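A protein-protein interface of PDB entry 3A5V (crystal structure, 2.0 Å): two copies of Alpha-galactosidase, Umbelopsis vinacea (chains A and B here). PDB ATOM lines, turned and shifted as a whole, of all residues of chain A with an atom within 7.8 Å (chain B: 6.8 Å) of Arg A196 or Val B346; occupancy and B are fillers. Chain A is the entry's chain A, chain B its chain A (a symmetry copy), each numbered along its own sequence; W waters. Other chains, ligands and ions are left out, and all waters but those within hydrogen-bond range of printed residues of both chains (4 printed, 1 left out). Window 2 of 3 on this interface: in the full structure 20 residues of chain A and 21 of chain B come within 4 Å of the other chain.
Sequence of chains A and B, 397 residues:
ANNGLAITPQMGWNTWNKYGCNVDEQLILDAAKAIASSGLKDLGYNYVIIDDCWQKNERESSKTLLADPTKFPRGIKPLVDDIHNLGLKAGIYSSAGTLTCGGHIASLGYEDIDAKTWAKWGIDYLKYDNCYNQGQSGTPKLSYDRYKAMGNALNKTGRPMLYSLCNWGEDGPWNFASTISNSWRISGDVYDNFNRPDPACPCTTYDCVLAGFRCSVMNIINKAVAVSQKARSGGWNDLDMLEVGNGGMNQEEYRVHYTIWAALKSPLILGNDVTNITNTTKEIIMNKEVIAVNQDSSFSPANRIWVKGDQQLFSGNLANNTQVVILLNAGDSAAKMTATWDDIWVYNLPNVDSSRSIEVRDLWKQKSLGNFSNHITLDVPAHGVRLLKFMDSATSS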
ATOM      1  N   TYR A 191      15.274 -14.666   5.337  1.00  0.00           N
ATOM      2  CA  TYR A 191      14.555 -13.719   4.501  1.00  0.00           C
ATOM      3  C   TYR A 191      14.384 -14.272   3.095  1.00  0.00           C
ATOM      4  O   TYR A 191      14.943 -15.336   2.763  1.00  0.00           O
ATOM      5  CB  TYR A 191      15.183 -12.322   4.492  1.00  0.00           C
ATOM      6  CG  TYR A 191      16.505 -12.129   3.769  1.00  0.00           C
ATOM      7  CD1 TYR A 191      17.584 -13.007   3.936  1.00  0.00           C
ATOM      8  CD2 TYR A 191      16.695 -10.989   2.972  1.00  0.00           C
ATOM      9  CE1 TYR A 191      18.834 -12.761   3.286  1.00  0.00           C
ATOM     10  CE2 TYR A 191      17.893 -10.736   2.341  1.00  0.00           C
ATOM     11  CZ  TYR A 191      18.961 -11.622   2.495  1.00  0.00           C
ATOM     12  OH  TYR A 191      20.134 -11.321   1.844  1.00  0.00           O
ATOM     13  N   ASP A 192      13.615 -13.553   2.274  1.00  0.00           N
ATOM     14  CA  ASP A 192      13.187 -14.073   0.972  1.00  0.00           C
ATOM     15  C   ASP A 192      14.318 -13.925  -0.038  1.00  0.00           C
ATOM     16  O   ASP A 192      14.215 -13.158  -1.012  1.00  0.00           O
ATOM     17  CB  ASP A 192      11.919 -13.331   0.515  1.00  0.00           C
ATOM     18  CG  ASP A 192      11.224 -14.003  -0.655  1.00  0.00           C
ATOM     19  OD1 ASP A 192      11.567 -15.155  -1.010  1.00  0.00           O
ATOM     20  OD2 ASP A 192      10.326 -13.354  -1.227  1.00  0.00           O
ATOM     21  N   ASN A 193      15.407 -14.651   0.202  1.00  0.00           N
ATOM     22  CA  ASN A 193      16.608 -14.521  -0.604  1.00  0.00           C
ATOM     23  C   ASN A 193      17.475 -15.777  -0.535  1.00  0.00           C
ATOM     24  O   ASN A 193      17.745 -16.298   0.561  1.00  0.00           O
ATOM     25  CB  ASN A 193      17.403 -13.299  -0.130  1.00  0.00           C
ATOM     26  CG  ASN A 193      18.477 -12.889  -1.116  1.00  0.00           C
ATOM     27  OD1 ASN A 193      19.415 -13.645  -1.366  1.00  0.00           O
ATOM     28  ND2 ASN A 193      18.348 -11.677  -1.679  1.00  0.00           N
ATOM     29  N   PHE A 194      17.934 -16.264  -1.689  1.00  0.00           N
ATOM     30  CA  PHE A 194      18.586 -17.587  -1.711  1.00  0.00           C
ATOM     31  C   PHE A 194      19.979 -17.636  -1.088  1.00  0.00           C
ATOM     32  O   PHE A 194      20.299 -18.589  -0.365  1.00  0.00           O
ATOM     33  CB  PHE A 194      18.623 -18.207  -3.125  1.00  0.00           C
ATOM     34  CG  PHE A 194      19.189 -19.621  -3.150  1.00  0.00           C
ATOM     35  CD1 PHE A 194      18.418 -20.702  -2.709  1.00  0.00           C
ATOM     36  CD2 PHE A 194      20.500 -19.851  -3.573  1.00  0.00           C
ATOM     37  CE1 PHE A 194      18.937 -22.010  -2.705  1.00  0.00           C
ATOM     38  CE2 PHE A 194      21.036 -21.147  -3.592  1.00  0.00           C
ATOM     39  CZ  PHE A 194      20.247 -22.236  -3.158  1.00  0.00           C
ATOM     40  N   ASN A 195      20.825 -16.637  -1.367  1.00  0.00           N
ATOM     41  CA  ASN A 195      22.213 -16.721  -0.905  1.00  0.00           C
ATOM     42  C   ASN A 195      22.938 -15.393  -0.598  1.00  0.00           C
ATOM     43  O   ASN A 195      24.137 -15.387  -0.307  1.00  0.00           O
ATOM     44  CB  ASN A 195      23.034 -17.591  -1.872  1.00  0.00           C
ATOM     45  CG  ASN A 195      23.198 -16.941  -3.244  1.00  0.00           C
ATOM     46  OD1 ASN A 195      22.856 -15.768  -3.439  1.00  0.00           O
ATOM     47  ND2 ASN A 195      23.746 -17.690  -4.185  1.00  0.00           N
ATOM     48  N   ARG A 196      22.221 -14.269  -0.643  1.00  0.00           N
ATOM     49  CA  ARG A 196      22.869 -12.977  -0.372  1.00  0.00           C
ATOM     50  C   ARG A 196      23.268 -12.846   1.112  1.00  0.00           C
ATOM     51  O   ARG A 196      22.396 -12.917   2.012  1.00  0.00           O
ATOM     52  CB  ARG A 196      21.963 -11.811  -0.792  1.00  0.00           C
ATOM     53  CG  ARG A 196      22.574 -10.419  -0.527  1.00  0.00           C
ATOM     54  CD  ARG A 196      21.575  -9.277  -0.774  1.00  0.00           C
ATOM     55  NE  ARG A 196      22.046  -8.042  -0.106  1.00  0.00           N
ATOM     56  CZ  ARG A 196      21.783  -7.724   1.157  1.00  0.00           C
ATOM     57  NH1 ARG A 196      21.018  -8.518   1.928  1.00  0.00           N
ATOM     58  NH2 ARG A 196      22.283  -6.607   1.657  1.00  0.00           N
ATOM     59  N   PRO A 197      24.570 -12.600   1.378  1.00  0.00           N
ATOM     60  CA  PRO A 197      24.973 -12.391   2.769  1.00  0.00           C
ATOM     61  C   PRO A 197      24.495 -11.013   3.246  1.00  0.00           C
ATOM     62  O   PRO A 197      24.257 -10.114   2.429  1.00  0.00           O
ATOM     63  CB  PRO A 197      26.503 -12.421   2.699  1.00  0.00           C
ATOM     64  CG  PRO A 197      26.810 -11.890   1.298  1.00  0.00           C
ATOM     65  CD  PRO A 197      25.702 -12.442   0.434  1.00  0.00           C
ATOM     66  N   ASP A 198      24.382 -10.832   4.553  1.00  0.00           N
ATOM     67  CA  ASP A 198      23.878  -9.558   5.070  1.00  0.00           C
ATOM     68  C   ASP A 198      24.565  -9.239   6.394  1.00  0.00           C
ATOM     69  O   ASP A 198      24.804 -10.161   7.192  1.00  0.00           O
ATOM     70  CB  ASP A 198      22.353  -9.663   5.275  1.00  0.00           C
ATOM     71  CG  ASP A 198      21.713  -8.327   5.537  1.00  0.00           C
ATOM     72  OD1 ASP A 198      21.665  -7.891   6.718  1.00  0.00           O
ATOM     73  OD2 ASP A 198      21.273  -7.689   4.557  1.00  0.00           O
ATOM     74  N   PRO A 199      24.885  -7.945   6.648  1.00  0.00           N
ATOM     75  CA  PRO A 199      25.630  -7.639   7.878  1.00  0.00           C
ATOM     76  C   PRO A 199      24.806  -7.865   9.149  1.00  0.00           C
ATOM     77  O   PRO A 199      25.387  -8.005  10.235  1.00  0.00           O
ATOM     78  CB  PRO A 199      25.995  -6.140   7.702  1.00  0.00           C
ATOM     79  CG  PRO A 199      24.845  -5.602   6.854  1.00  0.00           C
ATOM     80  CD  PRO A 199      24.685  -6.732   5.834  1.00  0.00           C
ATOM     81  N   ALA A 200      23.479  -7.921   9.017  1.00  0.00           N
ATOM     82  CA  ALA A 200      22.597  -8.234  10.163  1.00  0.00           C
ATOM     83  C   ALA A 200      22.581  -9.733  10.493  1.00  0.00           C
ATOM     84  O   ALA A 200      22.061 -10.130  11.531  1.00  0.00           O
ATOM     85  CB  ALA A 200      21.159  -7.701   9.930  1.00  0.00           C
ATOM     86  N   CYS A 201      23.140 -10.553   9.599  1.00  0.00           N
ATOM     87  CA  CYS A 201      23.308 -11.999   9.847  1.00  0.00           C
ATOM     88  C   CYS A 201      24.807 -12.362   9.728  1.00  0.00           C
ATOM     89  O   CYS A 201      25.225 -13.034   8.759  1.00  0.00           O
ATOM     90  CB  CYS A 201      22.448 -12.823   8.881  1.00  0.00           C
ATOM     91  SG  CYS A 201      22.533 -14.633   9.161  1.00  0.00           S
ATOM     92  N   ARG A 214      17.737 -11.478   8.332  1.00  0.00           N
ATOM     93  CA  ARG A 214      18.242 -11.430   6.945  1.00  0.00           C
ATOM     94  C   ARG A 214      19.344 -12.493   6.700  1.00  0.00           C
ATOM     95  O   ARG A 214      20.367 -12.223   6.048  1.00  0.00           O
ATOM     96  CB  ARG A 214      18.697 -10.002   6.568  1.00  0.00           C
ATOM     97  CG  ARG A 214      17.503  -9.023   6.605  1.00  0.00           C
ATOM     98  CD  ARG A 214      17.911  -7.541   6.758  1.00  0.00           C
ATOM     99  NE  ARG A 214      16.723  -6.667   6.698  1.00  0.00           N
ATOM    100  CZ  ARG A 214      16.700  -5.389   7.089  1.00  0.00           C
ATOM    101  NH1 ARG A 214      17.789  -4.818   7.598  1.00  0.00           N
ATOM    102  NH2 ARG A 214      15.567  -4.695   7.009  1.00  0.00           N
ATOM    103  N   CYS A 215      19.116 -13.699   7.225  1.00  0.00           N
ATOM    104  CA  CYS A 215      19.955 -14.864   6.913  1.00  0.00           C
ATOM    105  C   CYS A 215      19.404 -15.567   5.672  1.00  0.00           C
ATOM    106  O   CYS A 215      18.255 -15.982   5.659  1.00  0.00           O
ATOM    107  CB  CYS A 215      19.993 -15.857   8.090  1.00  0.00           C
ATOM    108  SG  CYS A 215      20.617 -15.151   9.645  1.00  0.00           S
ATOM    109  N   SER A 216      20.244 -15.721   4.644  1.00  0.00           N
ATOM    110  CA  SER A 216      19.829 -16.373   3.411  1.00  0.00           C
ATOM    111  C   SER A 216      19.520 -17.866   3.628  1.00  0.00           C
ATOM    112  O   SER A 216      19.905 -18.475   4.648  1.00  0.00           O
ATOM    113  CB  SER A 216      20.906 -16.197   2.327  1.00  0.00           C
ATOM    114  OG  SER A 216      22.012 -17.053   2.585  1.00  0.00           O
ATOM    115  N   VAL A 217      18.802 -18.451   2.670  1.00  0.00           N
ATOM    116  CA  VAL A 217      18.559 -19.902   2.672  1.00  0.00           C
ATOM    117  C   VAL A 217      19.877 -20.692   2.858  1.00  0.00           C
ATOM    118  O   VAL A 217      19.973 -21.550   3.753  1.00  0.00           O
ATOM    119  CB  VAL A 217      17.799 -20.325   1.372  1.00  0.00           C
ATOM    120  CG1 VAL A 217      17.709 -21.858   1.221  1.00  0.00           C
ATOM    121  CG2 VAL A 217      16.399 -19.698   1.383  1.00  0.00           C
ATOM    122  N   MET A 218      20.892 -20.369   2.047  1.00  0.00           N
ATOM    123  CA  MET A 218      22.178 -21.070   2.096  1.00  0.00           C
ATOM    124  C   MET A 218      22.916 -20.860   3.435  1.00  0.00           C
ATOM    125  O   MET A 218      23.532 -21.790   3.979  1.00  0.00           O
ATOM    126  CB  MET A 218      23.076 -20.677   0.903  1.00  0.00           C
ATOM    127  CG  MET A 218      22.605 -21.251  -0.459  1.00  0.00           C
ATOM    128  SD  MET A 218      22.441 -23.064  -0.458  1.00  0.00           S
ATOM    129  CE  MET A 218      24.097 -23.573   0.011  1.00  0.00           C
ATOM    130  N   ASN A 219      22.831 -19.645   3.970  1.00  0.00           N
ATOM    131  CA  ASN A 219      23.392 -19.360   5.301  1.00  0.00           C
ATOM    132  C   ASN A 219      22.792 -20.303   6.352  1.00  0.00           C
ATOM    133  O   ASN A 219      23.512 -20.924   7.148  1.00  0.00           O
ATOM    134  CB  ASN A 219      23.164 -17.871   5.676  1.00  0.00           C
ATOM    135  CG  ASN A 219      23.611 -17.540   7.099  1.00  0.00           C
ATOM    136  OD1 ASN A 219      22.909 -17.853   8.079  1.00  0.00           O
ATOM    137  ND2 ASN A 219      24.778 -16.889   7.225  1.00  0.00           N
ATOM    138  N   GLY A 248      10.895 -13.134  -3.910  1.00  0.00           N
ATOM    139  CA  GLY A 248      12.323 -12.756  -3.914  1.00  0.00           C
ATOM    140  C   GLY A 248      13.247 -13.903  -4.323  1.00  0.00           C
ATOM    141  O   GLY A 248      14.449 -13.709  -4.471  1.00  0.00           O
ATOM    142  N   ARG B 304      24.049  -1.414   5.761  1.00  0.00           N
ATOM    143  CA  ARG B 304      25.077  -1.633   4.739  1.00  0.00           C
ATOM    144  C   ARG B 304      24.593  -2.724   3.754  1.00  0.00           C
ATOM    145  O   ARG B 304      24.454  -3.895   4.117  1.00  0.00           O
ATOM    146  CB  ARG B 304      26.449  -1.984   5.354  1.00  0.00           C
ATOM    147  CG  ARG B 304      27.581  -2.091   4.309  1.00  0.00           C
ATOM    148  CD  ARG B 304      28.968  -1.963   4.932  1.00  0.00           C
ATOM    149  NE  ARG B 304      29.463  -3.208   5.525  1.00  0.00           N
ATOM    150  CZ  ARG B 304      30.559  -3.297   6.288  1.00  0.00           C
ATOM    151  NH1 ARG B 304      31.272  -2.212   6.600  1.00  0.00           N
ATOM    152  NH2 ARG B 304      30.922  -4.474   6.777  1.00  0.00           N
ATOM    153  N   ILE B 305      24.346  -2.320   2.518  1.00  0.00           N
ATOM    154  CA  ILE B 305      23.739  -3.171   1.493  1.00  0.00           C
ATOM    155  C   ILE B 305      24.777  -4.101   0.853  1.00  0.00           C
ATOM    156  O   ILE B 305      24.502  -5.283   0.645  1.00  0.00           O
ATOM    157  CB  ILE B 305      23.052  -2.307   0.394  1.00  0.00           C
ATOM    158  CG1 ILE B 305      21.995  -1.401   1.033  1.00  0.00           C
ATOM    159  CG2 ILE B 305      22.420  -3.193  -0.723  1.00  0.00           C
ATOM    160  CD1 ILE B 305      21.000  -2.153   1.965  1.00  0.00           C
ATOM    161  N   TRP B 306      25.960  -3.569   0.567  1.00  0.00           N
ATOM    162  CA  TRP B 306      27.066  -4.397   0.086  1.00  0.00           C
ATOM    163  C   TRP B 306      28.433  -3.822   0.390  1.00  0.00           C
ATOM    164  O   TRP B 306      28.577  -2.631   0.724  1.00  0.00           O
ATOM    165  CB  TRP B 306      26.960  -4.726  -1.423  1.00  0.00           C
ATOM    166  CG  TRP B 306      26.708  -3.585  -2.417  1.00  0.00           C
ATOM    167  CD1 TRP B 306      25.579  -3.421  -3.168  1.00  0.00           C
ATOM    168  CD2 TRP B 306      27.618  -2.535  -2.834  1.00  0.00           C
ATOM    169  NE1 TRP B 306      25.714  -2.341  -4.011  1.00  0.00           N
ATOM    170  CE2 TRP B 306      26.943  -1.765  -3.809  1.00  0.00           C
ATOM    171  CE3 TRP B 306      28.920  -2.156  -2.457  1.00  0.00           C
ATOM    172  CZ2 TRP B 306      27.531  -0.648  -4.434  1.00  0.00           C
ATOM    173  CZ3 TRP B 306      29.507  -1.042  -3.072  1.00  0.00           C
ATOM    174  CH2 TRP B 306      28.804  -0.296  -4.050  1.00  0.00           C
ATOM    175  N   SER B 315      22.009   2.222   2.802  1.00  0.00           N
ATOM    176  CA  SER B 315      20.662   2.649   2.426  1.00  0.00           C
ATOM    177  C   SER B 315      19.743   2.531   3.631  1.00  0.00           C
ATOM    178  O   SER B 315      19.736   1.493   4.308  1.00  0.00           O
ATOM    179  CB  SER B 315      20.139   1.761   1.288  1.00  0.00           C
ATOM    180  OG  SER B 315      18.801   2.082   0.974  1.00  0.00           O
ATOM    181  N   THR B 340      22.278   0.894  -7.546  1.00  0.00           N
ATOM    182  CA  THR B 340      21.106   0.553  -8.349  1.00  0.00           C
ATOM    183  C   THR B 340      19.860   0.630  -7.451  1.00  0.00           C
ATOM    184  O   THR B 340      19.964   0.532  -6.231  1.00  0.00           O
ATOM    185  CB  THR B 340      21.207  -0.861  -8.938  1.00  0.00           C
ATOM    186  OG1 THR B 340      21.030  -1.827  -7.898  1.00  0.00           O
ATOM    187  CG2 THR B 340      22.591  -1.089  -9.600  1.00  0.00           C
ATOM    188  N   TRP B 341      18.698   0.812  -8.067  1.00  0.00           N
ATOM    189  CA  TRP B 341      17.433   0.862  -7.341  1.00  0.00           C
ATOM    190  C   TRP B 341      17.183  -0.485  -6.655  1.00  0.00           C
ATOM    191  O   TRP B 341      16.670  -0.521  -5.523  1.00  0.00           O
ATOM    192  CB  TRP B 341      16.282   1.191  -8.315  1.00  0.00           C
ATOM    193  CG  TRP B 341      16.069   2.687  -8.705  1.00  0.00           C
ATOM    194  CD1 TRP B 341      14.889   3.243  -9.146  1.00  0.00           C
ATOM    195  CD2 TRP B 341      17.037   3.767  -8.703  1.00  0.00           C
ATOM    196  NE1 TRP B 341      15.064   4.583  -9.423  1.00  0.00           N
ATOM    197  CE2 TRP B 341      16.364   4.931  -9.151  1.00  0.00           C
ATOM    198  CE3 TRP B 341      18.406   3.864  -8.364  1.00  0.00           C
ATOM    199  CZ2 TRP B 341      17.010   6.177  -9.263  1.00  0.00           C
ATOM    200  CZ3 TRP B 341      19.043   5.093  -8.463  1.00  0.00           C
ATOM    201  CH2 TRP B 341      18.349   6.240  -8.922  1.00  0.00           C
ATOM    202  N   ASP B 342      17.539  -1.595  -7.325  1.00  0.00           N
ATOM    203  CA  ASP B 342      17.317  -2.909  -6.720  1.00  0.00           C
ATOM    204  C   ASP B 342      18.172  -3.102  -5.454  1.00  0.00           C
ATOM    205  O   ASP B 342      17.762  -3.817  -4.540  1.00  0.00           O
ATOM    206  CB  ASP B 342      17.540  -4.063  -7.711  1.00  0.00           C
ATOM    207  CG  ASP B 342      16.413  -4.172  -8.741  1.00  0.00           C
ATOM    208  OD1 ASP B 342      15.333  -3.543  -8.556  1.00  0.00           O
ATOM    209  OD2 ASP B 342      16.618  -4.887  -9.733  1.00  0.00           O
ATOM    210  N   ASP B 343      19.357  -2.502  -5.422  1.00  0.00           N
ATOM    211  CA  ASP B 343      20.187  -2.576  -4.212  1.00  0.00           C
ATOM    212  C   ASP B 343      19.686  -1.632  -3.120  1.00  0.00           C
ATOM    213  O   ASP B 343      19.595  -2.037  -1.962  1.00  0.00           O
ATOM    214  CB  ASP B 343      21.639  -2.281  -4.533  1.00  0.00           C
ATOM    215  CG  ASP B 343      22.343  -3.484  -5.172  1.00  0.00           C
ATOM    216  OD1 ASP B 343      21.908  -4.647  -4.960  1.00  0.00           O
ATOM    217  OD2 ASP B 343      23.323  -3.249  -5.877  1.00  0.00           O
ATOM    218  N   ILE B 344      19.366  -0.393  -3.491  1.00  0.00           N
ATOM    219  CA  ILE B 344      18.869   0.605  -2.526  1.00  0.00           C
ATOM    220  C   ILE B 344      17.649   0.084  -1.747  1.00  0.00           C
ATOM    221  O   ILE B 344      17.556   0.283  -0.519  1.00  0.00           O
ATOM    222  CB  ILE B 344      18.586   1.976  -3.205  1.00  0.00           C
ATOM    223  CG1 ILE B 344      19.915   2.594  -3.692  1.00  0.00           C
ATOM    224  CG2 ILE B 344      17.862   2.959  -2.230  1.00  0.00           C
ATOM    225  CD1 ILE B 344      19.753   3.710  -4.765  1.00  0.00           C
ATOM    226  N   TRP B 345      16.730  -0.580  -2.464  1.00  0.00           N
ATOM    227  CA  TRP B 345      15.537  -1.186  -1.852  1.00  0.00           C
ATOM    228  C   TRP B 345      15.578  -2.735  -1.862  1.00  0.00           C
ATOM    229  O   TRP B 345      14.541  -3.400  -2.032  1.00  0.00           O
ATOM    230  CB  TRP B 345      14.248  -0.641  -2.519  1.00  0.00           C
ATOM    231  CG  TRP B 345      14.039   0.822  -2.178  1.00  0.00           C
ATOM    232  CD1 TRP B 345      13.531   1.318  -1.016  1.00  0.00           C
ATOM    233  CD2 TRP B 345      14.368   1.952  -2.987  1.00  0.00           C
ATOM    234  NE1 TRP B 345      13.506   2.690  -1.051  1.00  0.00           N
ATOM    235  CE2 TRP B 345      14.014   3.111  -2.248  1.00  0.00           C
ATOM    236  CE3 TRP B 345      14.924   2.107  -4.267  1.00  0.00           C
ATOM    237  CZ2 TRP B 345      14.203   4.404  -2.738  1.00  0.00           C
ATOM    238  CZ3 TRP B 345      15.117   3.394  -4.761  1.00  0.00           C
ATOM    239  CH2 TRP B 345      14.743   4.531  -3.997  1.00  0.00           C
ATOM    240  N   VAL B 346      16.771  -3.303  -1.650  1.00  0.00           N
ATOM    241  CA  VAL B 346      16.937  -4.767  -1.665  1.00  0.00           C
ATOM    242  C   VAL B 346      15.930  -5.530  -0.779  1.00  0.00           C
ATOM    243  O   VAL B 346      15.411  -6.560  -1.202  1.00  0.00           O
ATOM    244  CB  VAL B 346      18.418  -5.225  -1.357  1.00  0.00           C
ATOM    245  CG1 VAL B 346      18.904  -4.752   0.037  1.00  0.00           C
ATOM    246  CG2 VAL B 346      18.590  -6.758  -1.536  1.00  0.00           C
ATOM    247  N   TYR B 347      15.646  -5.029   0.429  1.00  0.00           N
ATOM    248  CA  TYR B 347      14.790  -5.767   1.358  1.00  0.00           C
ATOM    249  C   TYR B 347      13.329  -5.772   0.902  1.00  0.00           C
ATOM    250  O   TYR B 347      12.523  -6.582   1.385  1.00  0.00           O
ATOM    251  CB  TYR B 347      14.959  -5.266   2.800  1.00  0.00           C
ATOM    252  CG  TYR B 347      16.423  -5.294   3.228  1.00  0.00           C
ATOM    253  CD1 TYR B 347      17.160  -6.489   3.188  1.00  0.00           C
ATOM    254  CD2 TYR B 347      17.071  -4.126   3.636  1.00  0.00           C
ATOM    255  CE1 TYR B 347      18.512  -6.510   3.537  1.00  0.00           C
ATOM    256  CE2 TYR B 347      18.410  -4.143   4.024  1.00  0.00           C
ATOM    257  CZ  TYR B 347      19.122  -5.334   3.953  1.00  0.00           C
ATOM    258  OH  TYR B 347      20.439  -5.338   4.319  1.00  0.00           O
ATOM    259  N   ASN B 348      13.007  -4.886  -0.044  1.00  0.00           N
ATOM    260  CA  ASN B 348      11.667  -4.855  -0.643  1.00  0.00           C
ATOM    261  C   ASN B 348      11.497  -5.724  -1.882  1.00  0.00           C
ATOM    262  O   ASN B 348      10.387  -5.837  -2.391  1.00  0.00           O
ATOM    263  CB  ASN B 348      11.248  -3.421  -0.984  1.00  0.00           C
ATOM    264  CG  ASN B 348      11.093  -2.552   0.245  1.00  0.00           C
ATOM    265  OD1 ASN B 348      11.982  -1.759   0.573  1.00  0.00           O
ATOM    266  ND2 ASN B 348       9.960  -2.677   0.919  1.00  0.00           N
ATOM    267  N   LEU B 349      12.578  -6.311  -2.394  1.00  0.00           N
ATOM    268  CA  LEU B 349      12.466  -7.127  -3.612  1.00  0.00           C
ATOM    269  C   LEU B 349      11.456  -8.272  -3.413  1.00  0.00           C
ATOM    270  O   LEU B 349      11.400  -8.863  -2.324  1.00  0.00           O
ATOM    271  CB  LEU B 349      13.837  -7.670  -4.035  1.00  0.00           C
ATOM    272  CG  LEU B 349      14.807  -6.620  -4.572  1.00  0.00           C
ATOM    273  CD1 LEU B 349      16.198  -7.221  -4.686  1.00  0.00           C
ATOM    274  CD2 LEU B 349      14.328  -6.049  -5.933  1.00  0.00           C
ATOM    275  N   PRO B 350      10.667  -8.608  -4.461  1.00  0.00           N
ATOM    276  CA  PRO B 350      10.713  -8.132  -5.836  1.00  0.00           C
ATOM    277  C   PRO B 350       9.890  -6.852  -6.100  1.00  0.00           C
ATOM    278  O   PRO B 350       9.775  -6.434  -7.256  1.00  0.00           O
ATOM    279  CB  PRO B 350      10.084  -9.301  -6.586  1.00  0.00           C
ATOM    280  CG  PRO B 350       8.946  -9.700  -5.659  1.00  0.00           C
ATOM    281  CD  PRO B 350       9.601  -9.619  -4.279  1.00  0.00           C
ATOM    282  N   VAL B 352       9.926  -3.693  -6.368  1.00  0.00           N
ATOM    283  CA  VAL B 352      10.706  -2.494  -6.640  1.00  0.00           C
ATOM    284  C   VAL B 352      10.591  -2.221  -8.120  1.00  0.00           C
ATOM    285  O   VAL B 352      10.768  -3.118  -8.956  1.00  0.00           O
ATOM    286  CB  VAL B 352      12.211  -2.647  -6.234  1.00  0.00           C
ATOM    287  CG1 VAL B 352      13.025  -1.380  -6.639  1.00  0.00           C
ATOM    288  CG2 VAL B 352      12.352  -2.961  -4.719  1.00  0.00           C
HETATM  289  O   HOH W   1      25.612  -8.028   1.249  1.00  0.00           O
HETATM  290  O   HOH W   2      23.542  -6.590  -2.034  1.00  0.00           O
HETATM  291  O   HOH W   3      13.500  -9.888  -0.597  1.00  0.00           O
HETATM  292  O   HOH W   4      20.690  -5.447   7.243  1.00  0.00           O
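Of the 16 printed residues of chain B, 5 touch a printed residue of chain A.
Hydrophobic or aromatic side chains of chain A that line the printed part of chain B: Pro A199.
Among the printed residues, no Asp or Glu carboxylate lies within 4 Å of a Lys or Arg side-chain nitrogen of the other chain.
Arg A196 touches three residues of chain B.
Of chain A, only Arg A196 (3.95 Å) comes within 4 Å of Val B346.
Of the printed residues of chain B, Asp A198 touches Tyr B347 (2.5 Å).
Of the printed residues of chain B, Arg A214 touches Tyr B347 (3.4 Å).
Of the printed residues of chain A, Tyr B347 touches Arg A196 (3.5 Å), Asp A198 (2.5 Å) and Arg A214 (3.4 Å).
Printed residues of chain B within 4 Å of Pro A199: Arg B304.
Ala A200 touches none of the printed residues of chain B.
Cys A215 touches none of the printed residues of chain B.
The nearest residue of chain A that does not touch Val B346 is Asn A193 (4.9 Å).
The nearest printed residue of chain B that does not touch Gly A248 is Leu B349 (4.3 Å).
OH of Tyr A191 is in hydrogen-bond range of O of Arg A196 (2.8 Å).
N of Gly A248 lies within hydrogen-bond range of OD2 of Asp A192, 2.8 Å away.
The backbone NH (N) of Arg A196 lies within hydrogen-bond range of the side-chain amide oxygen (OD1) of Asn A193, at 3.0 Å.
NH1 of Arg A196 is in salt-bridge range of OD2 of Asp A198 (2.8 Å).
The backbone NH (N) of Ala A200 sits at hydrogen-bond distance from the side-chain carboxylate (OD1) of Asp A198 (2.9 Å).
The side-chain sulfur of Cys A215 forms a disulfide with the side-chain sulfur of Cys A201, at 2.0 Å.
Water W4 lies within hydrogen-bond range of the side-chain carboxylate (OD1) of Asp A198 (2.7 Å), the side-chain hydroxyl (OH) of Tyr B347 (2.9 Å) and the guanidinium group (NH1) of Arg A214 (3.0 Å).
Water W1 bridges the backbone carbonyl oxygen of Pro A197 (2.8 Å) and the backbone carbonyl oxygen of Ile B305 (3.0 Å).
Water W2 bridges NE of Arg A196 and O of Ile B305.
Water W3 lies within hydrogen-bond range of the backbone carbonyl oxygen (O) of Leu B349 (2.9 Å) and the backbone carbonyl oxygen (O) of Asp A192 (3.4 Å).
O of Ile B305 is in hydrogen-bond range of NH2 of Arg A196 (2.8 Å).
NH2 of Arg A196 lies within hydrogen-bond range of OH of Tyr B347, at 3.5 Å.
OD2 of Asp A198 is in hydrogen-bond range of OH of Tyr B347, at 2.5 Å.
Val B346 touches Arg A196.
Pro A199 touches Arg B304 (CG to O, 3.2 Å).
CD of Arg A214 touches CE1 of Tyr B347, at 3.4 Å.
Gly A248 touches Pro B350 (N to CD, 3.8 Å).
No position is printed for both chains.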
